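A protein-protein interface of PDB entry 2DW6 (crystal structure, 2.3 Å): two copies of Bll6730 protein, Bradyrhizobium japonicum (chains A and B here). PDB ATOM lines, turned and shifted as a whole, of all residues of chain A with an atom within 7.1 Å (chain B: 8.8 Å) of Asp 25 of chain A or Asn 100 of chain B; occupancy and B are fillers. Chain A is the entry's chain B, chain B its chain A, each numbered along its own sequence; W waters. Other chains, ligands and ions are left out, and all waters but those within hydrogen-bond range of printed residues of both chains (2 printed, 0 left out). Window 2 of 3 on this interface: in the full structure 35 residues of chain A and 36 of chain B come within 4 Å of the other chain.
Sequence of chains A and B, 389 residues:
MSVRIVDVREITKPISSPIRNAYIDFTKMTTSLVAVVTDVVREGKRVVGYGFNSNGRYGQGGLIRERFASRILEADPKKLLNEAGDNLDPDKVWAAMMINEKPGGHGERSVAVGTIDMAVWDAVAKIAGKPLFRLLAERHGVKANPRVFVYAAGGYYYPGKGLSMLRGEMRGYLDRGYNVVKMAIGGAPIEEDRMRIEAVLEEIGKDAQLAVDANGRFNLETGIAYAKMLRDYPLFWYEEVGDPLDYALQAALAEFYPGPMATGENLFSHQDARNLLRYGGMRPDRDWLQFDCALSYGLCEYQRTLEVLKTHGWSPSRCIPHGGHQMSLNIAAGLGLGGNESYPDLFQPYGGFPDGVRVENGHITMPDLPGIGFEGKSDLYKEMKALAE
The side-chain amide oxygen (OD1) of Asn 100 of chain B lies close to the side-chain carboxylate (OD2) of Asp 25 of chain A (3.2 Å). OH of Tyr 58 of chain A is in hydrogen-bond range of O of Asn 100 of chain B (2.6 Å). The guanidinium group of Arg 71 of chain B sits at hydrogen-bond distance from the side-chain hydroxyl of Tyr 58 of chain A.
The backbone carbonyl oxygen (O) of Ile 99 of chain B lies close to the guanidinium group (NH1) of Arg 71 of chain B, at 3.3 Å. The side-chain amide oxygen of Asn 21 of chain A lies within hydrogen-bond range of the backbone NH of Ile 24 of chain A, at 2.7 Å. NH1 of Arg 71 of chain B lies within hydrogen-bond range of O of Met 97 of chain B, at 2.9 Å. The side-chain carboxylate (OD1) of Asp 25 of chain A is in hydrogen-bond range of the backbone NH (N) of Thr 27 of chain A (2.7 Å). The backbone NH (N) of Tyr 58 of chain A lies within hydrogen-bond range of the side-chain sulfur (SD) of Met 29 of chain A (3.7 Å). The guanidinium group (NH1) of Arg 67 of chain B is in salt-bridge range of the side-chain carboxylate (OE1) of Glu 101 of chain B (2.9 Å).
O of Glu 101 of chain B touches CE2 of Tyr 23 of chain A, at 3.6 Å. Pro 103 of chain B touches Tyr 23 of chain A. Asn 100 of chain B touches Ile 24 of chain A. Ile 24 of chain A touches Glu 101 of chain B (CD1 to O, 2.9 Å). N of Lys 102 of chain B touches CD1 of Ile 24 of chain A, 3.7 Å away. Lys 102 of chain B touches Gly 56 of chain A. CD2 of Tyr 58 of chain A touches CZ of Arg 67 of chain B, at 3.6 Å. OE2 of Glu 101 of chain B touches CE2 of Tyr 58 of chain A (3.8 Å).
Of chain B, only Asn 100 comes within 4 Å of Asp 25 of chain A. Asn 100 of chain B touches just these residues of chain A: Ile 24, Asp 25 and Tyr 58. Of the printed residues of chain B, Ile 24 of chain A touches Asn 100 (3.1 Å), Glu 101 (2.9 Å) and Lys 102 (3.7 Å). Of the printed residues of chain B, Tyr 23 of chain A touches Glu 101 (3.6 Å) and Pro 103 (3.6 Å). Printed residues of chain A within 4 Å of Pro 103 of chain B: Tyr 23 (3.6 Å). Of the printed residues of chain B, Gly 56 of chain A touches Lys 102. Pro 18 of chain A touches none of the printed residues of chain B.
Hydrophobic or aromatic side chains of chain A that line the printed part of chain B: Tyr 23, Ile 24 and Tyr 58. Hydrophobic or aromatic side chains of chain B that line the printed part of chain A: Pro 103.
No position is printed for both chains. Of the 11 pairs that touch across the chains among the printed residues, none has its exchanged pair printed and touching as well.
Water W1 lies within hydrogen-bond range of N of Lys 102 of chain B, O of Gly 56 of chain A and NH1 of Arg 109 of chain B. Water W2 bridges O of Tyr 23 of chain A and N of Asn 100 of chain B.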
ATOM      1  N   SER A  17      23.356  -9.187   4.079  1.00  0.00           N
ATOM      2  CA  SER A  17      22.903  -7.935   4.678  1.00  0.00           C
ATOM      3  C   SER A  17      22.342  -7.086   3.536  1.00  0.00           C
ATOM      4  O   SER A  17      22.594  -7.366   2.365  1.00  0.00           O
ATOM      5  CB  SER A  17      24.063  -7.191   5.343  1.00  0.00           C
ATOM      6  OG  SER A  17      24.934  -6.649   4.364  1.00  0.00           O
ATOM      7  N   PRO A  18      21.576  -6.039   3.861  1.00  0.00           N
ATOM      8  CA  PRO A  18      21.012  -5.200   2.799  1.00  0.00           C
ATOM      9  C   PRO A  18      21.945  -4.199   2.115  1.00  0.00           C
ATOM     10  O   PRO A  18      21.476  -3.310   1.408  1.00  0.00           O
ATOM     11  CB  PRO A  18      19.829  -4.525   3.486  1.00  0.00           C
ATOM     12  CG  PRO A  18      20.296  -4.409   4.906  1.00  0.00           C
ATOM     13  CD  PRO A  18      20.956  -5.738   5.163  1.00  0.00           C
ATOM     14  N   ILE A  19      23.258  -4.327   2.309  1.00  0.00           N
ATOM     15  CA  ILE A  19      24.170  -3.409   1.633  1.00  0.00           C
ATOM     16  C   ILE A  19      23.949  -3.584   0.135  1.00  0.00           C
ATOM     17  O   ILE A  19      23.592  -4.670  -0.334  1.00  0.00           O
ATOM     18  CB  ILE A  19      25.662  -3.686   1.954  1.00  0.00           C
ATOM     19  CG1 ILE A  19      26.057  -5.098   1.519  1.00  0.00           C
ATOM     20  CG2 ILE A  19      25.916  -3.469   3.428  1.00  0.00           C
ATOM     21  CD1 ILE A  19      27.569  -5.368   1.586  1.00  0.00           C
ATOM     22  N   ARG A  20      24.168  -2.517  -0.618  1.00  0.00           N
ATOM     23  CA  ARG A  20      23.958  -2.566  -2.052  1.00  0.00           C
ATOM     24  C   ARG A  20      24.994  -1.755  -2.813  1.00  0.00           C
ATOM     25  O   ARG A  20      25.475  -0.734  -2.317  1.00  0.00           O
ATOM     26  CB  ARG A  20      22.553  -2.032  -2.362  1.00  0.00           C
ATOM     27  CG  ARG A  20      22.237  -1.851  -3.837  1.00  0.00           C
ATOM     28  CD  ARG A  20      20.819  -1.319  -4.018  1.00  0.00           C
ATOM     29  NE  ARG A  20      20.659   0.022  -3.458  1.00  0.00           N
ATOM     30  CZ  ARG A  20      20.949   1.148  -4.107  1.00  0.00           C
ATOM     31  NH1 ARG A  20      21.413   1.109  -5.353  1.00  0.00           N
ATOM     32  NH2 ARG A  20      20.781   2.320  -3.507  1.00  0.00           N
ATOM     33  N   ASN A  21      25.362  -2.232  -3.999  1.00  0.00           N
ATOM     34  CA  ASN A  21      26.286  -1.494  -4.849  1.00  0.00           C
ATOM     35  C   ASN A  21      25.552  -1.272  -6.181  1.00  0.00           C
ATOM     36  O   ASN A  21      24.384  -1.639  -6.312  1.00  0.00           O
ATOM     37  CB  ASN A  21      27.633  -2.230  -5.042  1.00  0.00           C
ATOM     38  CG  ASN A  21      27.490  -3.586  -5.710  1.00  0.00           C
ATOM     39  OD1 ASN A  21      26.709  -3.755  -6.646  1.00  0.00           O
ATOM     40  ND2 ASN A  21      28.274  -4.561  -5.246  1.00  0.00           N
ATOM     41  N   ALA A  22      26.216  -0.676  -7.161  1.00  0.00           N
ATOM     42  CA  ALA A  22      25.569  -0.382  -8.440  1.00  0.00           C
ATOM     43  C   ALA A  22      24.981  -1.579  -9.174  1.00  0.00           C
ATOM     44  O   ALA A  22      24.035  -1.433  -9.947  1.00  0.00           O
ATOM     45  CB  ALA A  22      26.546   0.346  -9.355  1.00  0.00           C
ATOM     46  N   TYR A  23      25.519  -2.762  -8.918  1.00  0.00           N
ATOM     47  CA  TYR A  23      25.078  -3.959  -9.622  1.00  0.00           C
ATOM     48  C   TYR A  23      24.261  -4.965  -8.818  1.00  0.00           C
ATOM     49  O   TYR A  23      23.318  -5.567  -9.341  1.00  0.00           O
ATOM     50  CB  TYR A  23      26.309  -4.682 -10.176  1.00  0.00           C
ATOM     51  CG  TYR A  23      26.135  -5.308 -11.542  1.00  0.00           C
ATOM     52  CD1 TYR A  23      26.776  -4.768 -12.660  1.00  0.00           C
ATOM     53  CD2 TYR A  23      25.356  -6.450 -11.718  1.00  0.00           C
ATOM     54  CE1 TYR A  23      26.649  -5.348 -13.915  1.00  0.00           C
ATOM     55  CE2 TYR A  23      25.223  -7.041 -12.975  1.00  0.00           C
ATOM     56  CZ  TYR A  23      25.875  -6.482 -14.066  1.00  0.00           C
ATOM     57  OH  TYR A  23      25.756  -7.055 -15.308  1.00  0.00           O
ATOM     58  N   ILE A  24      24.610  -5.124  -7.547  1.00  0.00           N
ATOM     59  CA  ILE A  24      23.984  -6.133  -6.698  1.00  0.00           C
ATOM     60  C   ILE A  24      23.694  -5.698  -5.257  1.00  0.00           C
ATOM     61  O   ILE A  24      24.187  -4.662  -4.803  1.00  0.00           O
ATOM     62  CB  ILE A  24      24.948  -7.380  -6.692  1.00  0.00           C
ATOM     63  CG1 ILE A  24      24.304  -8.524  -7.449  1.00  0.00           C
ATOM     64  CG2 ILE A  24      25.385  -7.776  -5.286  1.00  0.00           C
ATOM     65  CD1 ILE A  24      24.189  -8.270  -8.917  1.00  0.00           C
ATOM     66  N   ASP A  25      22.856  -6.468  -4.557  1.00  0.00           N
ATOM     67  CA  ASP A  25      22.625  -6.216  -3.129  1.00  0.00           C
ATOM     68  C   ASP A  25      23.021  -7.558  -2.489  1.00  0.00           C
ATOM     69  O   ASP A  25      22.922  -8.606  -3.139  1.00  0.00           O
ATOM     70  CB  ASP A  25      21.170  -5.784  -2.801  1.00  0.00           C
ATOM     71  CG  ASP A  25      20.187  -6.944  -2.706  1.00  0.00           C
ATOM     72  OD1 ASP A  25      20.507  -7.983  -2.094  1.00  0.00           O
ATOM     73  OD2 ASP A  25      19.060  -6.800  -3.228  1.00  0.00           O
ATOM     74  N   PHE A  26      23.495  -7.527  -1.243  1.00  0.00           N
ATOM     75  CA  PHE A  26      23.974  -8.741  -0.564  1.00  0.00           C
ATOM     76  C   PHE A  26      22.972  -9.460   0.330  1.00  0.00           C
ATOM     77  O   PHE A  26      23.337 -10.137   1.296  1.00  0.00           O
ATOM     78  CB  PHE A  26      25.232  -8.397   0.232  1.00  0.00           C
ATOM     79  CG  PHE A  26      26.412  -8.070  -0.630  1.00  0.00           C
ATOM     80  CD1 PHE A  26      26.344  -7.042  -1.566  1.00  0.00           C
ATOM     81  CD2 PHE A  26      27.582  -8.812  -0.537  1.00  0.00           C
ATOM     82  CE1 PHE A  26      27.425  -6.761  -2.399  1.00  0.00           C
ATOM     83  CE2 PHE A  26      28.670  -8.538  -1.367  1.00  0.00           C
ATOM     84  CZ  PHE A  26      28.589  -7.508  -2.301  1.00  0.00           C
ATOM     85  N   THR A  27      21.708  -9.319  -0.033  1.00  0.00           N
ATOM     86  CA  THR A  27      20.587  -9.901   0.677  1.00  0.00           C
ATOM     87  C   THR A  27      20.634 -11.417   0.902  1.00  0.00           C
ATOM     88  O   THR A  27      20.151 -11.910   1.926  1.00  0.00           O
ATOM     89  CB  THR A  27      19.296  -9.485  -0.058  1.00  0.00           C
ATOM     90  OG1 THR A  27      18.757  -8.338   0.605  1.00  0.00           O
ATOM     91  CG2 THR A  27      18.276 -10.593  -0.113  1.00  0.00           C
ATOM     92  N   LYS A  28      21.214 -12.156  -0.039  1.00  0.00           N
ATOM     93  CA  LYS A  28      21.298 -13.607   0.083  1.00  0.00           C
ATOM     94  C   LYS A  28      22.743 -14.094  -0.032  1.00  0.00           C
ATOM     95  O   LYS A  28      22.982 -15.277  -0.262  1.00  0.00           O
ATOM     96  CB  LYS A  28      20.469 -14.272  -1.017  1.00  0.00           C
ATOM     97  CG  LYS A  28      18.996 -13.923  -1.025  1.00  0.00           C
ATOM     98  CD  LYS A  28      18.272 -14.614   0.120  1.00  0.00           C
ATOM     99  CE  LYS A  28      16.776 -14.730  -0.153  1.00  0.00           C
ATOM    100  NZ  LYS A  28      16.093 -13.406  -0.214  1.00  0.00           N
ATOM    101  N   MET A  29      23.705 -13.194   0.137  1.00  0.00           N
ATOM    102  CA  MET A  29      25.105 -13.577   0.000  1.00  0.00           C
ATOM    103  C   MET A  29      25.557 -14.643   0.992  1.00  0.00           C
ATOM    104  O   MET A  29      25.254 -14.581   2.186  1.00  0.00           O
ATOM    105  CB  MET A  29      26.011 -12.349   0.110  1.00  0.00           C
ATOM    106  CG  MET A  29      27.408 -12.571  -0.464  1.00  0.00           C
ATOM    107  SD  MET A  29      27.340 -13.272  -2.146  1.00  0.00           S
ATOM    108  CE  MET A  29      26.455 -11.968  -3.029  1.00  0.00           C
ATOM    109  N   GLY A  56      30.431 -11.972  -2.713  1.00  0.00           N
ATOM    110  CA  GLY A  56      30.007 -11.671  -4.065  1.00  0.00           C
ATOM    111  C   GLY A  56      29.634 -12.780  -5.021  1.00  0.00           C
ATOM    112  O   GLY A  56      28.720 -12.602  -5.823  1.00  0.00           O
ATOM    113  N   TYR A  58      28.865 -16.045  -4.020  1.00  0.00           N
ATOM    114  CA  TYR A  58      28.091 -17.076  -3.316  1.00  0.00           C
ATOM    115  C   TYR A  58      28.860 -18.359  -2.989  1.00  0.00           C
ATOM    116  O   TYR A  58      29.916 -18.639  -3.566  1.00  0.00           O
ATOM    117  CB  TYR A  58      26.842 -17.448  -4.117  1.00  0.00           C
ATOM    118  CG  TYR A  58      25.868 -16.309  -4.306  1.00  0.00           C
ATOM    119  CD1 TYR A  58      24.970 -15.954  -3.289  1.00  0.00           C
ATOM    120  CD2 TYR A  58      25.853 -15.569  -5.492  1.00  0.00           C
ATOM    121  CE1 TYR A  58      24.084 -14.890  -3.452  1.00  0.00           C
ATOM    122  CE2 TYR A  58      24.971 -14.501  -5.664  1.00  0.00           C
ATOM    123  CZ  TYR A  58      24.094 -14.165  -4.643  1.00  0.00           C
ATOM    124  OH  TYR A  58      23.242 -13.094  -4.792  1.00  0.00           O
ATOM    125  N   ARG B  67      19.769 -21.313  -5.961  1.00  0.00           N
ATOM    126  CA  ARG B  67      19.777 -19.916  -6.353  1.00  0.00           C
ATOM    127  C   ARG B  67      18.743 -19.415  -7.352  1.00  0.00           C
ATOM    128  O   ARG B  67      18.103 -18.378  -7.132  1.00  0.00           O
ATOM    129  CB  ARG B  67      21.175 -19.542  -6.858  1.00  0.00           C
ATOM    130  CG  ARG B  67      21.773 -18.346  -6.137  1.00  0.00           C
ATOM    131  CD  ARG B  67      22.953 -17.758  -6.889  1.00  0.00           C
ATOM    132  NE  ARG B  67      24.149 -18.543  -6.672  1.00  0.00           N
ATOM    133  CZ  ARG B  67      25.214 -18.520  -7.458  1.00  0.00           C
ATOM    134  NH1 ARG B  67      25.239 -17.744  -8.530  1.00  0.00           N
ATOM    135  NH2 ARG B  67      26.251 -19.290  -7.163  1.00  0.00           N
ATOM    136  N   PHE B  68      18.556 -20.145  -8.441  1.00  0.00           N
ATOM    137  CA  PHE B  68      17.642 -19.687  -9.472  1.00  0.00           C
ATOM    138  C   PHE B  68      16.162 -20.031  -9.372  1.00  0.00           C
ATOM    139  O   PHE B  68      15.320 -19.148  -9.521  1.00  0.00           O
ATOM    140  CB  PHE B  68      18.221 -20.093 -10.817  1.00  0.00           C
ATOM    141  CG  PHE B  68      19.612 -19.562 -11.029  1.00  0.00           C
ATOM    142  CD1 PHE B  68      19.829 -18.191 -11.154  1.00  0.00           C
ATOM    143  CD2 PHE B  68      20.711 -20.413 -11.014  1.00  0.00           C
ATOM    144  CE1 PHE B  68      21.122 -17.676 -11.255  1.00  0.00           C
ATOM    145  CE2 PHE B  68      22.004 -19.909 -11.113  1.00  0.00           C
ATOM    146  CZ  PHE B  68      22.213 -18.538 -11.232  1.00  0.00           C
ATOM    147  N   ARG B  71      14.303 -17.893  -6.750  1.00  0.00           N
ATOM    148  CA  ARG B  71      13.991 -16.516  -7.132  1.00  0.00           C
ATOM    149  C   ARG B  71      12.725 -16.446  -7.973  1.00  0.00           C
ATOM    150  O   ARG B  71      11.908 -15.544  -7.799  1.00  0.00           O
ATOM    151  CB  ARG B  71      15.154 -15.893  -7.901  1.00  0.00           C
ATOM    152  CG  ARG B  71      16.335 -15.543  -7.016  1.00  0.00           C
ATOM    153  CD  ARG B  71      17.568 -15.265  -7.844  1.00  0.00           C
ATOM    154  NE  ARG B  71      18.757 -15.052  -7.022  1.00  0.00           N
ATOM    155  CZ  ARG B  71      20.003 -15.185  -7.479  1.00  0.00           C
ATOM    156  NH1 ARG B  71      20.215 -15.531  -8.747  1.00  0.00           N
ATOM    157  NH2 ARG B  71      21.035 -14.976  -6.675  1.00  0.00           N
ATOM    158  N   GLU B  74       9.650 -17.189  -5.773  1.00  0.00           N
ATOM    159  CA  GLU B  74       9.441 -16.130  -4.790  1.00  0.00           C
ATOM    160  C   GLU B  74       9.007 -14.814  -5.420  1.00  0.00           C
ATOM    161  O   GLU B  74       8.570 -13.899  -4.722  1.00  0.00           O
ATOM    162  CB  GLU B  74      10.719 -15.902  -3.986  1.00  0.00           C
ATOM    163  CG  GLU B  74      11.046 -17.046  -3.043  1.00  0.00           C
ATOM    164  CD  GLU B  74      12.451 -16.956  -2.468  1.00  0.00           C
ATOM    165  OE1 GLU B  74      12.808 -17.830  -1.647  1.00  0.00           O
ATOM    166  OE2 GLU B  74      13.200 -16.021  -2.840  1.00  0.00           O
ATOM    167  N   ALA B  95      15.116 -12.085 -16.050  1.00  0.00           N
ATOM    168  CA  ALA B  95      15.576 -11.021 -15.178  1.00  0.00           C
ATOM    169  C   ALA B  95      15.359 -11.386 -13.715  1.00  0.00           C
ATOM    170  O   ALA B  95      16.226 -11.134 -12.871  1.00  0.00           O
ATOM    171  CB  ALA B  95      14.848  -9.726 -15.499  1.00  0.00           C
ATOM    172  N   ALA B  96      14.207 -11.981 -13.421  1.00  0.00           N
ATOM    173  CA  ALA B  96      13.886 -12.370 -12.057  1.00  0.00           C
ATOM    174  C   ALA B  96      14.892 -13.363 -11.483  1.00  0.00           C
ATOM    175  O   ALA B  96      15.286 -13.233 -10.326  1.00  0.00           O
ATOM    176  CB  ALA B  96      12.487 -12.952 -11.995  1.00  0.00           C
ATOM    177  N   MET B  97      15.320 -14.343 -12.275  1.00  0.00           N
ATOM    178  CA  MET B  97      16.257 -15.311 -11.737  1.00  0.00           C
ATOM    179  C   MET B  97      17.692 -14.816 -11.787  1.00  0.00           C
ATOM    180  O   MET B  97      18.577 -15.410 -11.186  1.00  0.00           O
ATOM    181  CB  MET B  97      16.099 -16.688 -12.418  1.00  0.00           C
ATOM    182  CG  MET B  97      16.569 -16.813 -13.841  1.00  0.00           C
ATOM    183  SD  MET B  97      16.330 -18.525 -14.426  1.00  0.00           S
ATOM    184  CE  MET B  97      15.677 -18.223 -16.090  1.00  0.00           C
ATOM    185  N   MET B  98      17.918 -13.700 -12.469  1.00  0.00           N
ATOM    186  CA  MET B  98      19.261 -13.139 -12.557  1.00  0.00           C
ATOM    187  C   MET B  98      19.548 -12.017 -11.556  1.00  0.00           C
ATOM    188  O   MET B  98      20.619 -11.419 -11.597  1.00  0.00           O
ATOM    189  CB  MET B  98      19.561 -12.639 -13.975  1.00  0.00           C
ATOM    190  CG  MET B  98      19.950 -13.740 -14.955  1.00  0.00           C
ATOM    191  SD  MET B  98      21.336 -14.764 -14.373  1.00  0.00           S
ATOM    192  CE  MET B  98      22.717 -13.643 -14.640  1.00  0.00           C
ATOM    193  N   ILE B  99      18.612 -11.723 -10.657  1.00  0.00           N
ATOM    194  CA  ILE B  99      18.860 -10.675  -9.668  1.00  0.00           C
ATOM    195  C   ILE B  99      19.974 -11.102  -8.717  1.00  0.00           C
ATOM    196  O   ILE B  99      20.141 -12.289  -8.417  1.00  0.00           O
ATOM    197  CB  ILE B  99      17.619 -10.359  -8.795  1.00  0.00           C
ATOM    198  CG1 ILE B  99      17.199 -11.607  -8.009  1.00  0.00           C
ATOM    199  CG2 ILE B  99      16.497  -9.830  -9.665  1.00  0.00           C
ATOM    200  CD1 ILE B  99      16.162 -11.356  -6.928  1.00  0.00           C
ATOM    201  N   ASN B 100      20.725 -10.118  -8.245  1.00  0.00           N
ATOM    202  CA  ASN B 100      21.823 -10.345  -7.313  1.00  0.00           C
ATOM    203  C   ASN B 100      22.928 -11.259  -7.832  1.00  0.00           C
ATOM    204  O   ASN B 100      23.571 -11.975  -7.064  1.00  0.00           O
ATOM    205  CB  ASN B 100      21.286 -10.863  -5.980  1.00  0.00           C
ATOM    206  CG  ASN B 100      20.360  -9.869  -5.313  1.00  0.00           C
ATOM    207  OD1 ASN B 100      20.582  -8.663  -5.387  1.00  0.00           O
ATOM    208  ND2 ASN B 100      19.320 -10.366  -4.651  1.00  0.00           N
ATOM    209  N   GLU B 101      23.143 -11.223  -9.143  1.00  0.00           N
ATOM    210  CA  GLU B 101      24.201 -12.000  -9.777  1.00  0.00           C
ATOM    211  C   GLU B 101      25.227 -10.984 -10.281  1.00  0.00           C
ATOM    212  O   GLU B 101      24.890 -10.121 -11.090  1.00  0.00           O
ATOM    213  CB  GLU B 101      23.654 -12.810 -10.955  1.00  0.00           C
ATOM    214  CG  GLU B 101      22.781 -13.994 -10.568  1.00  0.00           C
ATOM    215  CD  GLU B 101      23.515 -15.023  -9.721  1.00  0.00           C
ATOM    216  OE1 GLU B 101      24.668 -15.378 -10.056  1.00  0.00           O
ATOM    217  OE2 GLU B 101      22.930 -15.487  -8.722  1.00  0.00           O
ATOM    218  N   LYS B 102      26.466 -11.065  -9.795  1.00  0.00           N
ATOM    219  CA  LYS B 102      27.503 -10.124 -10.214  1.00  0.00           C
ATOM    220  C   LYS B 102      27.987 -10.447 -11.628  1.00  0.00           C
ATOM    221  O   LYS B 102      27.923 -11.599 -12.073  1.00  0.00           O
ATOM    222  CB  LYS B 102      28.685 -10.135  -9.235  1.00  0.00           C
ATOM    223  CG  LYS B 102      28.386  -9.457  -7.900  1.00  0.00           C
ATOM    224  CD  LYS B 102      29.595  -9.447  -6.957  1.00  0.00           C
ATOM    225  CE  LYS B 102      30.771  -8.664  -7.531  1.00  0.00           C
ATOM    226  NZ  LYS B 102      31.905  -8.539  -6.572  1.00  0.00           N
ATOM    227  N   PRO B 103      28.462  -9.421 -12.359  1.00  0.00           N
ATOM    228  CA  PRO B 103      28.960  -9.565 -13.731  1.00  0.00           C
ATOM    229  C   PRO B 103      30.192 -10.462 -13.856  1.00  0.00           C
ATOM    230  O   PRO B 103      30.911 -10.694 -12.879  1.00  0.00           O
ATOM    231  CB  PRO B 103      29.244  -8.122 -14.146  1.00  0.00           C
ATOM    232  CG  PRO B 103      29.624  -7.468 -12.842  1.00  0.00           C
ATOM    233  CD  PRO B 103      28.575  -8.021 -11.906  1.00  0.00           C
ATOM    234  N   ARG B 109      26.701 -21.327 -13.761  1.00  0.00           N
ATOM    235  CA  ARG B 109      25.413 -20.686 -13.545  1.00  0.00           C
ATOM    236  C   ARG B 109      24.763 -20.407 -14.905  1.00  0.00           C
ATOM    237  O   ARG B 109      23.542 -20.322 -15.019  1.00  0.00           O
ATOM    238  CB  ARG B 109      25.571 -19.388 -12.749  1.00  0.00           C
ATOM    239  CG  ARG B 109      26.259 -18.270 -13.490  1.00  0.00           C
ATOM    240  CD  ARG B 109      26.185 -16.970 -12.705  1.00  0.00           C
ATOM    241  NE  ARG B 109      26.795 -15.869 -13.444  1.00  0.00           N
ATOM    242  CZ  ARG B 109      26.963 -14.641 -12.967  1.00  0.00           C
ATOM    243  NH1 ARG B 109      26.567 -14.336 -11.737  1.00  0.00           N
ATOM    244  NH2 ARG B 109      27.542 -13.714 -13.719  1.00  0.00           N
HETATM  245  O   HOH W   1      27.494 -13.279  -8.554  1.00  0.00           O
HETATM  246  O   HOH W   2      20.837  -7.236  -9.191  1.00  0.00           O
